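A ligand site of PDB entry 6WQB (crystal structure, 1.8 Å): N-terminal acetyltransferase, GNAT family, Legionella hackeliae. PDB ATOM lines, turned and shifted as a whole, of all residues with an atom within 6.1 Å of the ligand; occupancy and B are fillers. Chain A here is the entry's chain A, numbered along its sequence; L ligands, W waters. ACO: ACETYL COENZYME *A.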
ATOM      1  N   CYS A  25       4.766 -25.681  13.035  1.00  0.00           N
ATOM      2  CA  CYS A  25       4.009 -26.242  14.156  1.00  0.00           C
ATOM      3  C   CYS A  25       3.105 -27.399  13.728  1.00  0.00           C
ATOM      4  O   CYS A  25       2.987 -28.394  14.456  1.00  0.00           O
ATOM      5  CB  CYS A  25       3.144 -25.184  14.830  1.00  0.00           C
ATOM      6  SG  CYS A  25       4.069 -23.845  15.644  1.00  0.00           S
ATOM      7  N   ASP A  29       2.930 -30.891  15.656  1.00  0.00           N
ATOM      8  CA  ASP A  29       1.818 -30.930  16.595  1.00  0.00           C
ATOM      9  C   ASP A  29       0.592 -31.638  16.038  1.00  0.00           C
ATOM     10  O   ASP A  29      -0.317 -31.976  16.825  1.00  0.00           O
ATOM     11  CB  ASP A  29       1.403 -29.506  16.985  1.00  0.00           C
ATOM     12  CG  ASP A  29       2.529 -28.706  17.609  1.00  0.00           C
ATOM     13  OD1 ASP A  29       3.476 -29.337  18.169  1.00  0.00           O
ATOM     14  OD2 ASP A  29       2.437 -27.437  17.601  1.00  0.00           O
ATOM     15  N   THR A  32      -3.118 -26.951  14.275  1.00  0.00           N
ATOM     16  CA  THR A  32      -2.718 -25.635  14.755  1.00  0.00           C
ATOM     17  C   THR A  32      -3.919 -24.992  15.455  1.00  0.00           C
ATOM     18  O   THR A  32      -5.060 -25.460  15.283  1.00  0.00           O
ATOM     19  CB  THR A  32      -2.291 -24.684  13.621  1.00  0.00           C
ATOM     20  OG1 THR A  32      -3.422 -24.339  12.827  1.00  0.00           O
ATOM     21  CG2 THR A  32      -1.194 -25.260  12.685  1.00  0.00           C
ATOM     22  N   PRO A  33      -3.692 -23.917  16.191  1.00  0.00           N
ATOM     23  CA  PRO A  33      -4.797 -23.029  16.588  1.00  0.00           C
ATOM     24  C   PRO A  33      -5.535 -22.494  15.368  1.00  0.00           C
ATOM     25  O   PRO A  33      -5.082 -22.552  14.219  1.00  0.00           O
ATOM     26  CB  PRO A  33      -4.097 -21.883  17.341  1.00  0.00           C
ATOM     27  CG  PRO A  33      -2.773 -22.543  17.850  1.00  0.00           C
ATOM     28  CD  PRO A  33      -2.390 -23.479  16.708  1.00  0.00           C
ATOM     29  N   LEU A  76      -2.199 -18.688  19.474  1.00  0.00           N
ATOM     30  CA  LEU A  76      -0.839 -18.496  19.949  1.00  0.00           C
ATOM     31  C   LEU A  76      -0.041 -19.697  19.486  1.00  0.00           C
ATOM     32  O   LEU A  76      -0.466 -20.827  19.731  1.00  0.00           O
ATOM     33  CB  LEU A  76      -0.824 -18.441  21.485  1.00  0.00           C
ATOM     34  CG  LEU A  76       0.454 -18.657  22.241  1.00  0.00           C
ATOM     35  CD1 LEU A  76       1.255 -17.441  21.995  1.00  0.00           C
ATOM     36  CD2 LEU A  76       0.143 -18.795  23.703  1.00  0.00           C
ATOM     37  N   ILE A  77       1.116 -19.441  18.852  1.00  0.00           N
ATOM     38  CA  ILE A  77       2.047 -20.519  18.420  1.00  0.00           C
ATOM     39  C   ILE A  77       3.472 -20.119  18.727  1.00  0.00           C
ATOM     40  O   ILE A  77       3.863 -18.945  18.575  1.00  0.00           O
ATOM     41  CB  ILE A  77       1.927 -20.834  16.904  1.00  0.00           C
ATOM     42  CG1 ILE A  77       2.074 -19.556  16.050  1.00  0.00           C
ATOM     43  CG2 ILE A  77       0.635 -21.648  16.554  1.00  0.00           C
ATOM     44  CD1 ILE A  77       2.005 -19.895  14.547  1.00  0.00           C
ATOM     45  N   VAL A  78       4.283 -21.107  19.154  1.00  0.00           N
ATOM     46  CA  VAL A  78       5.705 -20.952  19.378  1.00  0.00           C
ATOM     47  C   VAL A  78       6.434 -22.041  18.612  1.00  0.00           C
ATOM     48  O   VAL A  78       6.016 -23.221  18.627  1.00  0.00           O
ATOM     49  CB  VAL A  78       6.037 -21.003  20.893  1.00  0.00           C
ATOM     50  CG1 VAL A  78       7.562 -21.053  21.172  1.00  0.00           C
ATOM     51  CG2 VAL A  78       5.426 -19.747  21.586  1.00  0.00           C
ATOM     52  N   SER A  79       7.512 -21.670  17.960  1.00  0.00           N
ATOM     53  CA  SER A  79       8.320 -22.675  17.233  1.00  0.00           C
ATOM     54  C   SER A  79       8.592 -23.948  18.066  1.00  0.00           C
ATOM     55  O   SER A  79       9.090 -23.847  19.192  1.00  0.00           O
ATOM     56  CB  SER A  79       9.662 -22.069  16.811  1.00  0.00           C
ATOM     57  OG  SER A  79      10.540 -23.164  16.349  1.00  0.00           O
ATOM     58  N   HIS A  82      11.906 -24.156  20.032  1.00  0.00           N
ATOM     59  CA  HIS A  82      12.231 -23.127  21.016  1.00  0.00           C
ATOM     60  C   HIS A  82      11.193 -23.064  22.123  1.00  0.00           C
ATOM     61  O   HIS A  82      10.911 -21.979  22.641  1.00  0.00           O
ATOM     62  CB  HIS A  82      12.294 -21.747  20.353  1.00  0.00           C
ATOM     63  CG  HIS A  82      13.322 -21.679  19.284  1.00  0.00           C
ATOM     64  ND1 HIS A  82      14.625 -21.298  19.538  1.00  0.00           N
ATOM     65  CD2 HIS A  82      13.261 -21.998  17.968  1.00  0.00           C
ATOM     66  CE1 HIS A  82      15.308 -21.373  18.408  1.00  0.00           C
ATOM     67  NE2 HIS A  82      14.499 -21.773  17.441  1.00  0.00           N
ATOM     68  N   ARG A  83      10.622 -24.203  22.499  1.00  0.00           N
ATOM     69  CA  ARG A  83       9.541 -24.254  23.478  1.00  0.00           C
ATOM     70  C   ARG A  83      10.076 -24.402  24.885  1.00  0.00           C
ATOM     71  O   ARG A  83      11.227 -24.801  25.102  1.00  0.00           O
ATOM     72  CB  ARG A  83       8.582 -25.407  23.140  1.00  0.00           C
ATOM     73  CG  ARG A  83       7.770 -25.016  21.883  1.00  0.00           C
ATOM     74  CD  ARG A  83       6.676 -25.983  21.530  1.00  0.00           C
ATOM     75  NE  ARG A  83       5.977 -25.530  20.331  1.00  0.00           N
ATOM     76  CZ  ARG A  83       5.149 -26.329  19.666  1.00  0.00           C
ATOM     77  NH1 ARG A  83       4.978 -27.607  20.097  1.00  0.00           N
ATOM     78  NH2 ARG A  83       4.535 -25.906  18.564  1.00  0.00           N
ATOM     79  N   ARG A  84       9.216 -24.095  25.867  1.00  0.00           N
ATOM     80  CA  ARG A  84       9.596 -24.107  27.298  1.00  0.00           C
ATOM     81  C   ARG A  84      10.751 -23.162  27.582  1.00  0.00           C
ATOM     82  O   ARG A  84      11.629 -23.450  28.430  1.00  0.00           O
ATOM     83  CB  ARG A  84       9.928 -25.509  27.800  1.00  0.00           C
ATOM     84  CG  ARG A  84       8.794 -26.519  27.607  1.00  0.00           C
ATOM     85  CD  ARG A  84       7.504 -26.046  28.198  1.00  0.00           C
ATOM     86  NE  ARG A  84       7.458 -25.881  29.656  1.00  0.00           N
ATOM     87  CZ  ARG A  84       7.143 -26.847  30.506  1.00  0.00           C
ATOM     88  NH1 ARG A  84       6.916 -28.073  30.054  1.00  0.00           N
ATOM     89  NH2 ARG A  84       7.056 -26.588  31.806  1.00  0.00           N
ATOM     90  N   GLN A  85      10.789 -22.040  26.848  1.00  0.00           N
ATOM     91  CA  GLN A  85      11.757 -20.964  27.060  1.00  0.00           C
ATOM     92  C   GLN A  85      11.054 -19.672  27.484  1.00  0.00           C
ATOM     93  O   GLN A  85      11.735 -18.638  27.606  1.00  0.00           O
ATOM     94  CB  GLN A  85      12.557 -20.682  25.781  1.00  0.00           C
ATOM     95  CG  GLN A  85      13.595 -21.753  25.396  1.00  0.00           C
ATOM     96  CD  GLN A  85      14.288 -21.467  24.051  1.00  0.00           C
ATOM     97  OE1 GLN A  85      14.445 -20.321  23.637  1.00  0.00           O
ATOM     98  NE2 GLN A  85      14.722 -22.540  23.383  1.00  0.00           N
ATOM     99  N   GLY A  86       9.733 -19.711  27.673  1.00  0.00           N
ATOM    100  CA  GLY A  86       8.967 -18.572  28.137  1.00  0.00           C
ATOM    101  C   GLY A  86       8.526 -17.627  27.048  1.00  0.00           C
ATOM    102  O   GLY A  86       8.094 -16.506  27.363  1.00  0.00           O
ATOM    103  N   ILE A  87       8.606 -18.051  25.772  1.00  0.00           N
ATOM    104  CA  ILE A  87       8.130 -17.181  24.680  1.00  0.00           C
ATOM    105  C   ILE A  87       6.632 -16.947  24.770  1.00  0.00           C
ATOM    106  O   ILE A  87       6.155 -15.809  24.594  1.00  0.00           O
ATOM    107  CB  ILE A  87       8.526 -17.767  23.301  1.00  0.00           C
ATOM    108  CG1 ILE A  87      10.066 -17.777  23.154  1.00  0.00           C
ATOM    109  CG2 ILE A  87       7.794 -16.989  22.132  1.00  0.00           C
ATOM    110  CD1 ILE A  87      10.564 -18.445  21.837  1.00  0.00           C
ATOM    111  N   ALA A  88       5.835 -17.997  25.055  1.00  0.00           N
ATOM    112  CA  ALA A  88       4.390 -17.723  25.168  1.00  0.00           C
ATOM    113  C   ALA A  88       4.087 -16.812  26.354  1.00  0.00           C
ATOM    114  O   ALA A  88       3.187 -15.961  26.270  1.00  0.00           O
ATOM    115  CB  ALA A  88       3.595 -19.018  25.297  1.00  0.00           C
ATOM    116  N   LYS A  89       4.811 -16.995  27.455  1.00  0.00           N
ATOM    117  CA  LYS A  89       4.645 -16.064  28.572  1.00  0.00           C
ATOM    118  C   LYS A  89       4.970 -14.623  28.174  1.00  0.00           C
ATOM    119  O   LYS A  89       4.293 -13.681  28.625  1.00  0.00           O
ATOM    120  CB  LYS A  89       5.505 -16.487  29.775  1.00  0.00           C
ATOM    121  CG  LYS A  89       5.016 -17.808  30.394  1.00  0.00           C
ATOM    122  CD  LYS A  89       5.435 -18.009  31.882  1.00  0.00           C
ATOM    123  CE  LYS A  89       6.758 -18.760  32.014  1.00  0.00           C
ATOM    124  NZ  LYS A  89       6.898 -19.666  33.234  1.00  0.00           N
ATOM    125  N   GLN A  90       5.997 -14.439  27.326  1.00  0.00           N
ATOM    126  CA  GLN A  90       6.317 -13.080  26.871  1.00  0.00           C
ATOM    127  C   GLN A  90       5.209 -12.540  25.989  1.00  0.00           C
ATOM    128  O   GLN A  90       4.805 -11.374  26.139  1.00  0.00           O
ATOM    129  CB  GLN A  90       7.635 -13.052  26.083  1.00  0.00           C
ATOM    130  CG  GLN A  90       8.917 -13.051  26.907  1.00  0.00           C
ATOM    131  CD  GLN A  90      10.194 -12.745  26.097  1.00  0.00           C
ATOM    132  OE1 GLN A  90      10.413 -11.592  25.682  1.00  0.00           O
ATOM    133  NE2 GLN A  90      11.045 -13.776  25.913  1.00  0.00           N
ATOM    134  N   LEU A  92       1.998 -13.370  25.965  1.00  0.00           N
ATOM    135  CA  LEU A  92       0.810 -13.078  26.783  1.00  0.00           C
ATOM    136  C   LEU A  92       1.029 -11.863  27.656  1.00  0.00           C
ATOM    137  O   LEU A  92       0.094 -11.062  27.883  1.00  0.00           O
ATOM    138  CB  LEU A  92       0.461 -14.304  27.644  1.00  0.00           C
ATOM    139  CG  LEU A  92      -0.515 -15.196  26.841  1.00  0.00           C
ATOM    140  CD1 LEU A  92      -0.656 -16.549  27.451  1.00  0.00           C
ATOM    141  CD2 LEU A  92      -1.934 -14.550  26.714  1.00  0.00           C
ATOM    142  N   PHE A 109      -8.746 -20.260  24.307  1.00  0.00           N
ATOM    143  CA  PHE A 109      -7.584 -20.596  23.473  1.00  0.00           C
ATOM    144  C   PHE A 109      -7.994 -21.719  22.542  1.00  0.00           C
ATOM    145  O   PHE A 109      -8.605 -22.708  22.992  1.00  0.00           O
ATOM    146  CB  PHE A 109      -6.376 -21.080  24.302  1.00  0.00           C
ATOM    147  CG  PHE A 109      -5.709 -20.004  25.096  1.00  0.00           C
ATOM    148  CD1 PHE A 109      -6.206 -19.663  26.340  1.00  0.00           C
ATOM    149  CD2 PHE A 109      -4.552 -19.389  24.626  1.00  0.00           C
ATOM    150  CE1 PHE A 109      -5.592 -18.638  27.131  1.00  0.00           C
ATOM    151  CE2 PHE A 109      -3.925 -18.392  25.406  1.00  0.00           C
ATOM    152  CZ  PHE A 109      -4.463 -18.005  26.665  1.00  0.00           C
ATOM    153  N   SER A 110      -7.652 -21.594  21.269  1.00  0.00           N
ATOM    154  CA  SER A 110      -7.749 -22.712  20.345  1.00  0.00           C
ATOM    155  C   SER A 110      -6.423 -23.468  20.392  1.00  0.00           C
ATOM    156  O   SER A 110      -5.356 -22.848  20.500  1.00  0.00           O
ATOM    157  CB  SER A 110      -8.043 -22.257  18.896  1.00  0.00           C
ATOM    158  OG  SER A 110      -7.188 -21.231  18.403  1.00  0.00           O
ATOM    159  N   THR A 111      -6.475 -24.791  20.249  1.00  0.00           N
ATOM    160  CA  THR A 111      -5.260 -25.597  20.358  1.00  0.00           C
ATOM    161  C   THR A 111      -5.351 -26.776  19.405  1.00  0.00           C
ATOM    162  O   THR A 111      -6.455 -27.241  19.086  1.00  0.00           O
ATOM    163  CB  THR A 111      -5.070 -26.091  21.809  1.00  0.00           C
ATOM    164  OG1 THR A 111      -3.856 -26.911  21.916  1.00  0.00           O
ATOM    165  CG2 THR A 111      -6.251 -26.985  22.270  1.00  0.00           C
ATOM    166  N   PRO A 112      -4.228 -27.264  18.885  1.00  0.00           N
ATOM    167  CA  PRO A 112      -4.229 -28.586  18.269  1.00  0.00           C
ATOM    168  C   PRO A 112      -4.777 -29.586  19.281  1.00  0.00           C
ATOM    169  O   PRO A 112      -4.615 -29.425  20.489  1.00  0.00           O
ATOM    170  CB  PRO A 112      -2.748 -28.849  17.967  1.00  0.00           C
ATOM    171  CG  PRO A 112      -1.991 -27.885  18.869  1.00  0.00           C
ATOM    172  CD  PRO A 112      -2.879 -26.676  18.984  1.00  0.00           C
ATOM    173  N   ILE A 115      -2.251 -32.867  22.318  1.00  0.00           N
ATOM    174  CA  ILE A 115      -0.881 -32.690  22.827  1.00  0.00           C
ATOM    175  C   ILE A 115      -0.851 -31.876  24.116  1.00  0.00           C
ATOM    176  O   ILE A 115       0.094 -31.985  24.898  1.00  0.00           O
ATOM    177  CB  ILE A 115       0.036 -32.060  21.738  1.00  0.00           C
ATOM    178  CG1 ILE A 115      -0.459 -30.669  21.319  1.00  0.00           C
ATOM    179  CG2 ILE A 115       0.044 -32.915  20.518  1.00  0.00           C
ATOM    180  CD1 ILE A 115       0.556 -29.876  20.480  1.00  0.00           C
ATOM    181  N   ASN A 116      -1.844 -31.030  24.363  1.00  0.00           N
ATOM    182  CA  ASN A 116      -1.823 -30.170  25.540  1.00  0.00           C
ATOM    183  C   ASN A 116      -2.803 -30.599  26.608  1.00  0.00           C
ATOM    184  O   ASN A 116      -2.863 -29.944  27.652  1.00  0.00           O
ATOM    185  CB  ASN A 116      -2.148 -28.691  25.159  1.00  0.00           C
ATOM    186  CG  ASN A 116      -1.060 -28.068  24.295  1.00  0.00           C
ATOM    187  OD1 ASN A 116       0.137 -28.268  24.580  1.00  0.00           O
ATOM    188  ND2 ASN A 116      -1.451 -27.359  23.195  1.00  0.00           N
ATOM    189  N   TRP A 119      -1.738 -30.837  30.548  1.00  0.00           N
ATOM    190  CA  TRP A 119      -1.437 -29.723  31.410  1.00  0.00           C
ATOM    191  C   TRP A 119      -2.547 -28.673  31.396  1.00  0.00           C
ATOM    192  O   TRP A 119      -2.705 -27.944  32.387  1.00  0.00           O
ATOM    193  CB  TRP A 119      -0.078 -29.115  31.037  1.00  0.00           C
ATOM    194  CG  TRP A 119       0.014 -28.485  29.678  1.00  0.00           C
ATOM    195  CD1 TRP A 119       0.478 -29.077  28.543  1.00  0.00           C
ATOM    196  CD2 TRP A 119      -0.268 -27.120  29.335  1.00  0.00           C
ATOM    197  NE1 TRP A 119       0.487 -28.161  27.511  1.00  0.00           N
ATOM    198  CE2 TRP A 119       0.031 -26.958  27.980  1.00  0.00           C
ATOM    199  CE3 TRP A 119      -0.739 -26.019  30.070  1.00  0.00           C
ATOM    200  CZ2 TRP A 119      -0.148 -25.729  27.309  1.00  0.00           C
ATOM    201  CZ3 TRP A 119      -0.902 -24.802  29.414  1.00  0.00           C
ATOM    202  CH2 TRP A 119      -0.593 -24.670  28.057  1.00  0.00           C
ATOM    203  N   LEU A 120      -3.352 -28.632  30.330  1.00  0.00           N
ATOM    204  CA  LEU A 120      -4.478 -27.702  30.345  1.00  0.00           C
ATOM    205  C   LEU A 120      -5.422 -28.076  31.477  1.00  0.00           C
ATOM    206  O   LEU A 120      -5.921 -27.194  32.199  1.00  0.00           O
ATOM    207  CB  LEU A 120      -5.174 -27.715  29.008  1.00  0.00           C
ATOM    208  CG  LEU A 120      -4.370 -27.136  27.842  1.00  0.00           C
ATOM    209  CD1 LEU A 120      -5.056 -27.390  26.502  1.00  0.00           C
ATOM    210  CD2 LEU A 120      -4.301 -25.587  28.038  1.00  0.00           C
ATOM    211  N   GLN A 123      -3.971 -27.205  34.943  1.00  0.00           N
ATOM    212  CA  GLN A 123      -3.935 -25.773  35.205  1.00  0.00           C
ATOM    213  C   GLN A 123      -5.335 -25.165  35.217  1.00  0.00           C
ATOM    214  O   GLN A 123      -5.474 -23.929  35.220  1.00  0.00           O
ATOM    215  CB  GLN A 123      -3.056 -25.055  34.171  1.00  0.00           C
ATOM    216  CG  GLN A 123      -1.568 -25.344  34.430  1.00  0.00           C
ATOM    217  CD  GLN A 123      -0.625 -24.501  33.607  1.00  0.00           C
ATOM    218  OE1 GLN A 123      -0.984 -23.428  33.098  1.00  0.00           O
ATOM    219  NE2 GLN A 123       0.605 -24.983  33.464  1.00  0.00           N
ATOM    220  N   PHE A 125      -7.901 -25.157  32.931  1.00  0.00           N
ATOM    221  CA  PHE A 125      -8.654 -24.780  31.744  1.00  0.00           C
ATOM    222  C   PHE A 125      -9.817 -25.746  31.571  1.00  0.00           C
ATOM    223  O   PHE A 125      -9.752 -26.916  31.980  1.00  0.00           O
ATOM    224  CB  PHE A 125      -7.822 -24.844  30.474  1.00  0.00           C
ATOM    225  CG  PHE A 125      -6.657 -23.869  30.415  1.00  0.00           C
ATOM    226  CD1 PHE A 125      -5.480 -24.085  31.159  1.00  0.00           C
ATOM    227  CD2 PHE A 125      -6.717 -22.767  29.550  1.00  0.00           C
ATOM    228  CE1 PHE A 125      -4.398 -23.221  31.088  1.00  0.00           C
ATOM    229  CE2 PHE A 125      -5.629 -21.888  29.440  1.00  0.00           C
ATOM    230  CZ  PHE A 125      -4.497 -22.098  30.213  1.00  0.00           C
ATOM    231  N   LEU A 286      -5.184 -17.507  34.948  1.00  0.00           N
ATOM    232  CA  LEU A 286      -4.019 -17.646  34.072  1.00  0.00           C
ATOM    233  C   LEU A 286      -2.852 -16.812  34.577  1.00  0.00           C
ATOM    234  O   LEU A 286      -1.692 -17.273  34.553  1.00  0.00           O
ATOM    235  CB  LEU A 286      -4.401 -17.239  32.661  1.00  0.00           C
ATOM    236  CG  LEU A 286      -3.290 -17.271  31.604  1.00  0.00           C
ATOM    237  CD1 LEU A 286      -2.780 -18.694  31.298  1.00  0.00           C
ATOM    238  CD2 LEU A 286      -3.837 -16.626  30.336  1.00  0.00           C
ATOM    239  N   ASN A 289      -1.106 -18.799  37.342  1.00  0.00           N
ATOM    240  CA  ASN A 289      -0.481 -20.068  36.992  1.00  0.00           C
ATOM    241  C   ASN A 289       0.779 -19.850  36.162  1.00  0.00           C
ATOM    242  O   ASN A 289       1.694 -20.696  36.177  1.00  0.00           O
ATOM    243  CB  ASN A 289      -1.473 -20.978  36.256  1.00  0.00           C
ATOM    244  CG  ASN A 289      -2.821 -21.059  36.962  1.00  0.00           C
ATOM    245  OD1 ASN A 289      -3.014 -20.462  38.016  1.00  0.00           O
ATOM    246  ND2 ASN A 289      -3.752 -21.790  36.381  1.00  0.00           N
ATOM    247  N   TRP A 290       0.837 -18.739  35.433  1.00  0.00           N
ATOM    248  CA  TRP A 290       1.988 -18.414  34.606  1.00  0.00           C
ATOM    249  C   TRP A 290       2.781 -17.263  35.199  1.00  0.00           C
ATOM    250  O   TRP A 290       3.612 -16.652  34.514  1.00  0.00           O
ATOM    251  CB  TRP A 290       1.544 -18.078  33.184  1.00  0.00           C
ATOM    252  CG  TRP A 290       1.113 -19.268  32.384  1.00  0.00           C
ATOM    253  CD1 TRP A 290       0.685 -20.468  32.872  1.00  0.00           C
ATOM    254  CD2 TRP A 290       1.063 -19.377  30.956  1.00  0.00           C
ATOM    255  NE1 TRP A 290       0.378 -21.314  31.838  1.00  0.00           N
ATOM    256  CE2 TRP A 290       0.601 -20.662  30.653  1.00  0.00           C
ATOM    257  CE3 TRP A 290       1.375 -18.502  29.911  1.00  0.00           C
ATOM    258  CZ2 TRP A 290       0.436 -21.106  29.336  1.00  0.00           C
ATOM    259  CZ3 TRP A 290       1.214 -18.941  28.606  1.00  0.00           C
ATOM    260  CH2 TRP A 290       0.743 -20.231  28.331  1.00  0.00           C
HETATM  261  N1A ACO L   1       3.843 -29.299  29.204  1.00  0.00           N
HETATM  262  C2A ACO L   1       3.384 -28.768  30.309  1.00  0.00           C
HETATM  263  N3A ACO L   1       3.229 -27.495  30.462  1.00  0.00           N
HETATM  264  C4A ACO L   1       3.519 -26.641  29.502  1.00  0.00           C
HETATM  265  C5A ACO L   1       4.005 -27.140  28.251  1.00  0.00           C
HETATM  266  C6A ACO L   1       4.150 -28.589  28.151  1.00  0.00           C
HETATM  267  N6A ACO L   1       4.589 -29.148  27.046  1.00  0.00           N
HETATM  268  N7A ACO L   1       4.228 -26.124  27.464  1.00  0.00           N
HETATM  269  C8A ACO L   1       3.862 -25.060  28.175  1.00  0.00           C
HETATM  270  N9A ACO L   1       3.456 -25.360  29.378  1.00  0.00           N
HETATM  271  C1B ACO L   1       2.990 -24.433  30.395  1.00  0.00           C
HETATM  272  C2B ACO L   1       3.880 -24.375  31.611  1.00  0.00           C
HETATM  273  O2B ACO L   1       2.990 -23.929  32.604  1.00  0.00           O
HETATM  274  C3B ACO L   1       4.762 -23.230  31.274  1.00  0.00           C
HETATM  275  O3B ACO L   1       5.296 -22.668  32.432  1.00  0.00           O
HETATM  276  P3B ACO L   1       6.454 -23.366  33.200  1.00  0.00           P
HETATM  277  O7A ACO L   1       6.622 -22.293  34.161  1.00  0.00           O
HETATM  278  O8A ACO L   1       5.863 -24.596  33.714  1.00  0.00           O
HETATM  279  O9A ACO L   1       7.485 -23.586  32.225  1.00  0.00           O
HETATM  280  C4B ACO L   1       3.780 -22.272  30.626  1.00  0.00           C
HETATM  281  O4B ACO L   1       2.959 -23.122  29.881  1.00  0.00           O
HETATM  282  C5B ACO L   1       4.396 -21.252  29.725  1.00  0.00           C
HETATM  283  O5B ACO L   1       5.423 -21.800  29.016  1.00  0.00           O
HETATM  284  P1A ACO L   1       6.171 -21.172  27.892  1.00  0.00           P
HETATM  285  O1A ACO L   1       7.478 -21.588  27.880  1.00  0.00           O
HETATM  286  O2A ACO L   1       5.948 -19.773  27.926  1.00  0.00           O
HETATM  287  O3A ACO L   1       5.419 -21.812  26.639  1.00  0.00           O
HETATM  288  P2A ACO L   1       5.961 -21.950  25.219  1.00  0.00           P
HETATM  289  O4A ACO L   1       6.762 -20.925  24.730  1.00  0.00           O
HETATM  290  O5A ACO L   1       6.601 -23.196  25.186  1.00  0.00           O
HETATM  291  O6A ACO L   1       4.690 -22.076  24.283  1.00  0.00           O
HETATM  292  CBP ACO L   1       2.601 -23.184  23.741  1.00  0.00           C
HETATM  293  CCP ACO L   1       3.696 -22.936  24.714  1.00  0.00           C
HETATM  294  CDP ACO L   1       1.668 -24.268  24.061  1.00  0.00           C
HETATM  295  CEP ACO L   1       2.262 -22.079  22.807  1.00  0.00           C
HETATM  296  CAP ACO L   1       3.430 -23.978  22.672  1.00  0.00           C
HETATM  297  OAP ACO L   1       3.834 -25.314  23.049  1.00  0.00           O
HETATM  298  C9P ACO L   1       2.845 -24.127  21.255  1.00  0.00           C
HETATM  299  O9P ACO L   1       3.063 -23.366  20.405  1.00  0.00           O
HETATM  300  N8P ACO L   1       2.084 -25.153  21.033  1.00  0.00           N
HETATM  301  C7P ACO L   1       1.357 -25.267  19.787  1.00  0.00           C
HETATM  302  C6P ACO L   1       0.250 -24.234  19.675  1.00  0.00           C
HETATM  303  C5P ACO L   1      -0.749 -24.391  20.771  1.00  0.00           C
HETATM  304  O5P ACO L   1      -0.923 -25.445  21.248  1.00  0.00           O
HETATM  305  N4P ACO L   1      -1.360 -23.283  21.152  1.00  0.00           N
HETATM  306  C3P ACO L   1      -2.359 -23.248  22.161  1.00  0.00           C
HETATM  307  C2P ACO L   1      -1.847 -22.944  23.538  1.00  0.00           C
HETATM  308  S1P ACO L   1      -3.068 -22.881  24.755  1.00  0.00           S
HETATM  309  C   ACO L   1      -2.292 -21.962  25.869  1.00  0.00           C
HETATM  310  O   ACO L   1      -1.203 -21.571  25.692  1.00  0.00           O
HETATM  311  CH3 ACO L   1      -2.980 -21.621  27.125  1.00  0.00           C
HETATM  312  O   HOH W   1       8.933 -21.764  30.223  1.00  0.00           O
HETATM  313  O   HOH W   2       6.613 -28.209  24.868  1.00  0.00           O
HETATM  314  O   HOH W   3       5.672 -25.791  24.957  1.00  0.00           O
HETATM  315  O   HOH W   4       6.629 -26.553  35.642  1.00  0.00           O
HETATM  316  O   HOH W   5       9.282 -20.881  24.742  1.00  0.00           O
HETATM  317  O   HOH W   6       9.878 -24.774  32.700  1.00  0.00           O
HETATM  318  O   HOH W   7       3.200 -27.365  33.070  1.00  0.00           O
HETATM  319  O   HOH W   8       2.359 -27.800  22.934  1.00  0.00           O
HETATM  320  O   HOH W   9       0.262 -26.125  16.695  1.00  0.00           O
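Residues that only touch the ligand: Pro 112 (3.2 Å), Asp 29 (3.3 Å), Trp 290 (3.3 Å), Trp 119 (3.4 Å), Ser 110 (3.4 Å), Phe 125 (3.5 Å), Ile 87 (3.6 Å), Ile 77 (3.6 Å), Phe 109 (3.6 Å) and Pro 33 (3.7 Å).
21 residues have an atom within 4 Å of the ligand: Asp 29, Pro 33, Leu 76, Ile 77, Val 78, Arg 83, Arg 84, Gln 85, Gly 86, Ile 87, Ala 88, Lys 89, Phe 109, Ser 110, Thr 111, Pro 112, Asn 116, Trp 119, Gln 123, Phe 125 and Trp 290.
The guanidinium group (NH2) of Arg 84 is in salt-bridge range of an oxygen (O8A) of the ligand (3.0 Å).
An oxygen (O1A) of the ligand sits at hydrogen-bond distance from the backbone NH of Gly 86, 2.9 Å away.
An oxygen (O1A) of the ligand sits at hydrogen-bond distance from the backbone NH (N) of Gln 85 (3.5 Å).
An oxygen (O2B) of the ligand is in hydrogen-bond range of the side-chain amide nitrogen of Gln 123 (2.7 Å).
O5A of the ligand lies within hydrogen-bond range of N of Arg 84.
An oxygen (O2A) of the ligand is in hydrogen-bond range of the backbone NH of Lys 89 (3.0 Å).
The backbone carbonyl oxygen (O) of Leu 76 sits at hydrogen-bond distance from a nitrogen (N4P) of the ligand (3.0 Å).
O7A of the ligand lies within salt-bridge range of NZ of Lys 89, at 2.8 Å.
O9P of the ligand lies within hydrogen-bond range of N of Val 78, at 2.9 Å.
N of Ala 88 lies within hydrogen-bond range of O4A of the ligand (3.1 Å).
The side-chain hydroxyl (OG1) of Thr 111 is in hydrogen-bond range of an oxygen (O5P) of the ligand, 3.3 Å away.
ND2 of Asn 116 lies within hydrogen-bond range of O5P of the ligand.
The guanidinium group (NH2) of Arg 83 sits at hydrogen-bond distance from an oxygen (O9P) of the ligand, at 3.5 Å.
Water W6 lies within hydrogen-bond range of O9A of the ligand (2.7 Å) and NH2 of Arg 84 (3.5 Å).
Water W1 bridges O1A of the ligand (2.8 Å) and N of Gly 86 (3.4 Å).
Water W8 lies within hydrogen-bond range of the side-chain amide oxygen of Asn 116 and an oxygen (OAP) of the ligand.
The backbone carbonyl oxygen of Val 78 sits at hydrogen-bond distance from the side-chain sulfur of Cys 25, 3.6 Å away.
OD2 of Asp 29 is in salt-bridge range of NH2 of Arg 83, at 2.8 Å.
The backbone carbonyl oxygen (O) of Gln 123 is in hydrogen-bond range of the side-chain amide nitrogen (ND2) of Asn 289 (3.0 Å).
The backbone carbonyl oxygen (O) of Leu 120 is in hydrogen-bond range of the backbone NH (N) of Phe 125, at 2.9 Å.
The guanidinium group of Arg 83 is in hydrogen-bond range of the side-chain sulfur of Cys 25 (3.6 Å).
OG1 of Thr 111 lies within hydrogen-bond range of ND2 of Asn 116 (2.8 Å).
The indole nitrogen of Trp 290 is in hydrogen-bond range of the side-chain amide oxygen of Gln 123.
The side-chain amide oxygen of Asn 116 is in hydrogen-bond range of the indole nitrogen of Trp 119, 3.0 Å away.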
